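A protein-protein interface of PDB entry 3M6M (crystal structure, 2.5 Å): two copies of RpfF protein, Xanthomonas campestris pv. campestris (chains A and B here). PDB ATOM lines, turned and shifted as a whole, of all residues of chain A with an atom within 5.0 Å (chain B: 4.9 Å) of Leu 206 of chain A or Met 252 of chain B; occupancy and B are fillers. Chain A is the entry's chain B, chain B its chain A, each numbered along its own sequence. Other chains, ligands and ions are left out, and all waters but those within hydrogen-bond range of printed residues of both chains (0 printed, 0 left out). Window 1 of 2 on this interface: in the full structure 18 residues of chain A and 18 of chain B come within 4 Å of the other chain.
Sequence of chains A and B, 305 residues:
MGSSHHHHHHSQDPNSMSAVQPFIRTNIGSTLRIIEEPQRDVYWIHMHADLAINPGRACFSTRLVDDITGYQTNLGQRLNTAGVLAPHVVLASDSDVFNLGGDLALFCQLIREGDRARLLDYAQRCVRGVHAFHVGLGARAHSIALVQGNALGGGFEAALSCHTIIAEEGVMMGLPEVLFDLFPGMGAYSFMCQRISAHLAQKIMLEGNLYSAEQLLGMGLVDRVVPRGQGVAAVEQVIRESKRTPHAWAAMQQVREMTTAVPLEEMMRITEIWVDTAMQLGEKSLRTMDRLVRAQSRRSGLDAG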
ATOM      1  N   VAL A 178      21.355  20.694 -19.756  1.00  0.00           N
ATOM      2  CA  VAL A 178      22.198  21.602 -18.973  1.00  0.00           C
ATOM      3  C   VAL A 178      23.660  21.553 -19.379  1.00  0.00           C
ATOM      4  O   VAL A 178      24.383  22.531 -19.201  1.00  0.00           O
ATOM      5  CB  VAL A 178      22.112  21.365 -17.444  1.00  0.00           C
ATOM      6  CG1 VAL A 178      20.953  22.135 -16.860  1.00  0.00           C
ATOM      7  CG2 VAL A 178      22.030  19.883 -17.106  1.00  0.00           C
ATOM      8  N   PHE A 183      17.879  24.019 -20.704  1.00  0.00           N
ATOM      9  CA  PHE A 183      17.077  23.277 -19.735  1.00  0.00           C
ATOM     10  C   PHE A 183      15.964  22.501 -20.451  1.00  0.00           C
ATOM     11  O   PHE A 183      15.608  22.843 -21.580  1.00  0.00           O
ATOM     12  CB  PHE A 183      16.500  24.219 -18.666  1.00  0.00           C
ATOM     13  CG  PHE A 183      15.305  25.009 -19.126  1.00  0.00           C
ATOM     14  CD1 PHE A 183      14.014  24.574 -18.835  1.00  0.00           C
ATOM     15  CD2 PHE A 183      15.468  26.187 -19.849  1.00  0.00           C
ATOM     16  CE1 PHE A 183      12.899  25.297 -19.255  1.00  0.00           C
ATOM     17  CE2 PHE A 183      14.361  26.922 -20.274  1.00  0.00           C
ATOM     18  CZ  PHE A 183      13.071  26.477 -19.979  1.00  0.00           C
ATOM     19  N   GLN A 202      13.851  20.419  -9.660  1.00  0.00           N
ATOM     20  CA  GLN A 202      14.843  21.429 -10.025  1.00  0.00           C
ATOM     21  C   GLN A 202      16.276  20.891 -10.041  1.00  0.00           C
ATOM     22  O   GLN A 202      17.015  21.134 -10.995  1.00  0.00           O
ATOM     23  CB  GLN A 202      14.765  22.613  -9.066  1.00  0.00           C
ATOM     24  CG  GLN A 202      14.143  23.856  -9.643  1.00  0.00           C
ATOM     25  CD  GLN A 202      14.607  25.100  -8.910  1.00  0.00           C
ATOM     26  OE1 GLN A 202      15.517  25.801  -9.363  1.00  0.00           O
ATOM     27  NE2 GLN A 202      14.000  25.369  -7.752  1.00  0.00           N
ATOM     28  N   LYS A 203      16.662  20.177  -8.982  1.00  0.00           N
ATOM     29  CA  LYS A 203      17.989  19.555  -8.892  1.00  0.00           C
ATOM     30  C   LYS A 203      18.265  18.646 -10.077  1.00  0.00           C
ATOM     31  O   LYS A 203      19.296  18.772 -10.733  1.00  0.00           O
ATOM     32  CB  LYS A 203      18.126  18.732  -7.612  1.00  0.00           C
ATOM     33  CG  LYS A 203      18.669  19.476  -6.414  1.00  0.00           C
ATOM     34  CD  LYS A 203      18.967  18.487  -5.297  1.00  0.00           C
ATOM     35  CE  LYS A 203      18.794  19.124  -3.927  1.00  0.00           C
ATOM     36  NZ  LYS A 203      18.684  18.104  -2.841  1.00  0.00           N
ATOM     37  N   ILE A 204      17.334  17.731 -10.339  1.00  0.00           N
ATOM     38  CA  ILE A 204      17.478  16.749 -11.409  1.00  0.00           C
ATOM     39  C   ILE A 204      17.645  17.423 -12.768  1.00  0.00           C
ATOM     40  O   ILE A 204      18.451  16.979 -13.585  1.00  0.00           O
ATOM     41  CB  ILE A 204      16.292  15.743 -11.419  1.00  0.00           C
ATOM     42  CG1 ILE A 204      16.297  14.923 -10.122  1.00  0.00           C
ATOM     43  CG2 ILE A 204      16.360  14.822 -12.646  1.00  0.00           C
ATOM     44  CD1 ILE A 204      15.023  14.156  -9.858  1.00  0.00           C
ATOM     45  N   MET A 205      16.900  18.501 -12.991  1.00  0.00           N
ATOM     46  CA  MET A 205      16.975  19.254 -14.242  1.00  0.00           C
ATOM     47  C   MET A 205      18.299  19.984 -14.432  1.00  0.00           C
ATOM     48  O   MET A 205      18.728  20.192 -15.564  1.00  0.00           O
ATOM     49  CB  MET A 205      15.817  20.246 -14.345  1.00  0.00           C
ATOM     50  CG  MET A 205      14.476  19.595 -14.609  1.00  0.00           C
ATOM     51  SD  MET A 205      13.104  20.746 -14.429  1.00  0.00           S
ATOM     52  CE  MET A 205      13.143  21.573 -16.013  1.00  0.00           C
ATOM     53  N   LEU A 206      18.948  20.356 -13.330  1.00  0.00           N
ATOM     54  CA  LEU A 206      20.164  21.177 -13.391  1.00  0.00           C
ATOM     55  C   LEU A 206      21.473  20.438 -13.105  1.00  0.00           C
ATOM     56  O   LEU A 206      22.550  21.017 -13.240  1.00  0.00           O
ATOM     57  CB  LEU A 206      20.033  22.399 -12.474  1.00  0.00           C
ATOM     58  CG  LEU A 206      19.000  23.464 -12.861  1.00  0.00           C
ATOM     59  CD1 LEU A 206      18.820  24.478 -11.738  1.00  0.00           C
ATOM     60  CD2 LEU A 206      19.385  24.166 -14.164  1.00  0.00           C
ATOM     61  N   GLU A 207      21.386  19.170 -12.713  1.00  0.00           N
ATOM     62  CA  GLU A 207      22.587  18.378 -12.440  1.00  0.00           C
ATOM     63  C   GLU A 207      23.149  17.706 -13.686  1.00  0.00           C
ATOM     64  O   GLU A 207      24.361  17.594 -13.834  1.00  0.00           O
ATOM     65  CB  GLU A 207      22.336  17.342 -11.342  1.00  0.00           C
ATOM     66  CG  GLU A 207      22.472  17.900  -9.929  1.00  0.00           C
ATOM     67  CD  GLU A 207      22.357  16.832  -8.846  1.00  0.00           C
ATOM     68  OE1 GLU A 207      22.344  15.623  -9.174  1.00  0.00           O
ATOM     69  OE2 GLU A 207      22.280  17.210  -7.657  1.00  0.00           O
ATOM     70  N   GLY A 208      22.266  17.254 -14.572  1.00  0.00           N
ATOM     71  CA  GLY A 208      22.681  16.601 -15.811  1.00  0.00           C
ATOM     72  C   GLY A 208      23.244  15.208 -15.622  1.00  0.00           C
ATOM     73  O   GLY A 208      24.177  14.815 -16.323  1.00  0.00           O
ATOM     74  N   ALA B 248      21.097  28.194 -18.123  1.00  0.00           N
ATOM     75  CA  ALA B 248      20.186  27.181 -17.586  1.00  0.00           C
ATOM     76  C   ALA B 248      19.593  27.608 -16.243  1.00  0.00           C
ATOM     77  O   ALA B 248      18.394  27.434 -16.009  1.00  0.00           O
ATOM     78  CB  ALA B 248      20.888  25.835 -17.460  1.00  0.00           C
ATOM     79  N   TRP B 249      20.430  28.174 -15.374  1.00  0.00           N
ATOM     80  CA  TRP B 249      19.965  28.663 -14.077  1.00  0.00           C
ATOM     81  C   TRP B 249      18.931  29.781 -14.216  1.00  0.00           C
ATOM     82  O   TRP B 249      17.858  29.719 -13.610  1.00  0.00           O
ATOM     83  CB  TRP B 249      21.124  29.145 -13.193  1.00  0.00           C
ATOM     84  CG  TRP B 249      20.604  29.744 -11.925  1.00  0.00           C
ATOM     85  CD1 TRP B 249      20.364  31.068 -11.674  1.00  0.00           C
ATOM     86  CD2 TRP B 249      20.182  29.032 -10.755  1.00  0.00           C
ATOM     87  NE1 TRP B 249      19.840  31.224 -10.412  1.00  0.00           N
ATOM     88  CE2 TRP B 249      19.722  29.992  -9.824  1.00  0.00           C
ATOM     89  CE3 TRP B 249      20.160  27.676 -10.396  1.00  0.00           C
ATOM     90  CZ2 TRP B 249      19.242  29.639  -8.558  1.00  0.00           C
ATOM     91  CZ3 TRP B 249      19.688  27.324  -9.131  1.00  0.00           C
ATOM     92  CH2 TRP B 249      19.238  28.306  -8.228  1.00  0.00           C
ATOM     93  N   ALA B 250      19.272  30.800 -15.005  1.00  0.00           N
ATOM     94  CA  ALA B 250      18.422  31.976 -15.198  1.00  0.00           C
ATOM     95  C   ALA B 250      17.078  31.616 -15.817  1.00  0.00           C
ATOM     96  O   ALA B 250      16.046  32.172 -15.429  1.00  0.00           O
ATOM     97  CB  ALA B 250      19.140  33.025 -16.044  1.00  0.00           C
ATOM     98  N   ALA B 251      17.099  30.685 -16.770  1.00  0.00           N
ATOM     99  CA  ALA B 251      15.879  30.189 -17.402  1.00  0.00           C
ATOM    100  C   ALA B 251      14.990  29.468 -16.388  1.00  0.00           C
ATOM    101  O   ALA B 251      13.769  29.626 -16.408  1.00  0.00           O
ATOM    102  CB  ALA B 251      16.217  29.280 -18.558  1.00  0.00           C
ATOM    103  N   MET B 252      15.610  28.700 -15.494  1.00  0.00           N
ATOM    104  CA  MET B 252      14.882  27.971 -14.457  1.00  0.00           C
ATOM    105  C   MET B 252      14.190  28.895 -13.459  1.00  0.00           C
ATOM    106  O   MET B 252      13.118  28.566 -12.942  1.00  0.00           O
ATOM    107  CB  MET B 252      15.800  26.987 -13.732  1.00  0.00           C
ATOM    108  CG  MET B 252      15.916  25.631 -14.406  1.00  0.00           C
ATOM    109  SD  MET B 252      14.442  24.614 -14.173  1.00  0.00           S
ATOM    110  CE  MET B 252      13.468  25.071 -15.594  1.00  0.00           C
ATOM    111  N   GLN B 253      14.805  30.047 -13.194  1.00  0.00           N
ATOM    112  CA  GLN B 253      14.191  31.070 -12.349  1.00  0.00           C
ATOM    113  C   GLN B 253      12.932  31.645 -12.992  1.00  0.00           C
ATOM    114  O   GLN B 253      11.934  31.861 -12.306  1.00  0.00           O
ATOM    115  CB  GLN B 253      15.184  32.189 -12.012  1.00  0.00           C
ATOM    116  CG  GLN B 253      16.456  31.725 -11.304  1.00  0.00           C
ATOM    117  CD  GLN B 253      16.187  30.695 -10.222  1.00  0.00           C
ATOM    118  OE1 GLN B 253      16.490  29.509 -10.390  1.00  0.00           O
ATOM    119  NE2 GLN B 253      15.602  31.134  -9.113  1.00  0.00           N
ATOM    120  N   GLN B 254      12.982  31.873 -14.306  1.00  0.00           N
ATOM    121  CA  GLN B 254      11.817  32.329 -15.066  1.00  0.00           C
ATOM    122  C   GLN B 254      10.690  31.302 -14.995  1.00  0.00           C
ATOM    123  O   GLN B 254       9.518  31.670 -14.877  1.00  0.00           O
ATOM    124  CB  GLN B 254      12.177  32.588 -16.532  1.00  0.00           C
ATOM    125  CG  GLN B 254      13.185  33.702 -16.768  1.00  0.00           C
ATOM    126  CD  GLN B 254      13.523  33.878 -18.242  1.00  0.00           C
ATOM    127  OE1 GLN B 254      12.660  34.204 -19.056  1.00  0.00           O
ATOM    128  NE2 GLN B 254      14.786  33.660 -18.587  1.00  0.00           N
ATOM    129  N   VAL B 255      11.054  30.021 -15.061  1.00  0.00           N
ATOM    130  CA  VAL B 255      10.089  28.923 -14.985  1.00  0.00           C
ATOM    131  C   VAL B 255       9.462  28.864 -13.591  1.00  0.00           C
ATOM    132  O   VAL B 255       8.253  28.665 -13.456  1.00  0.00           O
ATOM    133  CB  VAL B 255      10.732  27.562 -15.374  1.00  0.00           C
ATOM    134  CG1 VAL B 255       9.774  26.398 -15.113  1.00  0.00           C
ATOM    135  CG2 VAL B 255      11.158  27.576 -16.836  1.00  0.00           C
ATOM    136  N   ARG B 256      10.290  29.052 -12.565  1.00  0.00           N
ATOM    137  CA  ARG B 256       9.812  29.153 -11.187  1.00  0.00           C
ATOM    138  C   ARG B 256       8.838  30.318 -11.018  1.00  0.00           C
ATOM    139  O   ARG B 256       7.755  30.140 -10.456  1.00  0.00           O
ATOM    140  CB  ARG B 256      10.978  29.309 -10.214  1.00  0.00           C
ATOM    141  CG  ARG B 256      11.749  28.029  -9.944  1.00  0.00           C
ATOM    142  CD  ARG B 256      13.017  28.312  -9.149  1.00  0.00           C
ATOM    143  NE  ARG B 256      12.751  28.493  -7.721  1.00  0.00           N
ATOM    144  CZ  ARG B 256      12.699  29.669  -7.096  1.00  0.00           C
ATOM    145  NH1 ARG B 256      12.902  30.804  -7.756  1.00  0.00           N
ATOM    146  NH2 ARG B 256      12.449  29.710  -5.796  1.00  0.00           N
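The guanidinium group (NE) of Arg 256 of chain B sits close to the side-chain amide nitrogen (NE2) of Gln 202 of chain A (3.4 Å).
No position is printed for both chains.
Of the 10 pairs that touch across the chains among the printed residues, none has its exchanged pair printed and touching as well.
Of the 9 printed residues of chain A, 5 touch a printed residue of chain B.
Printed residues of chain A that touch a printed residue of chain B: Val 178, Phe 183, Gln 202, Met 205 and Leu 206.
Hydrophobic or aromatic side chains of chain A that line the printed part of chain B: Val 178, Phe 183, Met 205 and Leu 206.
Printed residues of chain B that touch a printed residue of chain A: Ala 248, Trp 249, Ala 251, Met 252, Gln 253, Val 255 and Arg 256.
Hydrophobic or aromatic side chains of chain B that line the printed part of chain A: Ala 248, Trp 249, Ala 251, Met 252 and Val 255.
Among the printed residues, 10 pairs touch across the chains.
Printed residues of chain B within 4 Å of Phe 183 of chain A: Ala 251, Met 252 and Val 255.
Of the printed residues of chain B, Gln 202 of chain A touches Gln 253 (3.97 Å) and Arg 256 (3.4 Å).
Lys 203 of chain A touches none of the printed residues of chain B.
Printed residues of chain B within 4 Å of Met 205 of chain A: Met 252.
Of chain B, only Ala 248 (3.9 Å), Trp 249 (3.7 Å) and Met 252 (3.8 Å) come within 4 Å of Leu 206 of chain A.
Of the printed residues of chain A, Met 252 of chain B touches Phe 183, Met 205 and Leu 206.
Printed residues of chain A within 4 Å of Val 255 of chain B: Phe 183 (3.8 Å).
Of the printed residues of chain A, Arg 256 of chain B touches Gln 202 (3.4 Å).
The nearest printed residue of chain B that does not touch Leu 206 of chain A is Gln 253 of chain B (5.7 Å).
The nearest residue of chain A that does not touch Met 252 of chain B is Gln 202 of chain A (4.5 Å).
The nearest printed residue of chain B that does not touch Phe 183 of chain A is Ala 248 of chain B (4.6 Å).
Among the printed residues, pairs that only touch across the chains: Val 178 of chain A with Ala 248 of chain B (3.7 Å), Phe 183 of chain A with Ala 251 of chain B (3.4 Å), Phe 183 of chain A with Met 252 of chain B (3.3 Å), Phe 183 of chain A with Val 255 of chain B (3.8 Å), Gln 202 of chain A with Gln 253 of chain B (3.97 Å), Met 205 of chain A with Met 252 of chain B (3.5 Å), Leu 206 of chain A with Ala 248 of chain B (3.9 Å), Leu 206 of chain A with Trp 249 of chain B (3.7 Å) and Leu 206 of chain A with Met 252 of chain B (3.8 Å).
NE2 of Gln 253 of chain B lies close to NH1 of Arg 256 of chain B (3.0 Å).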
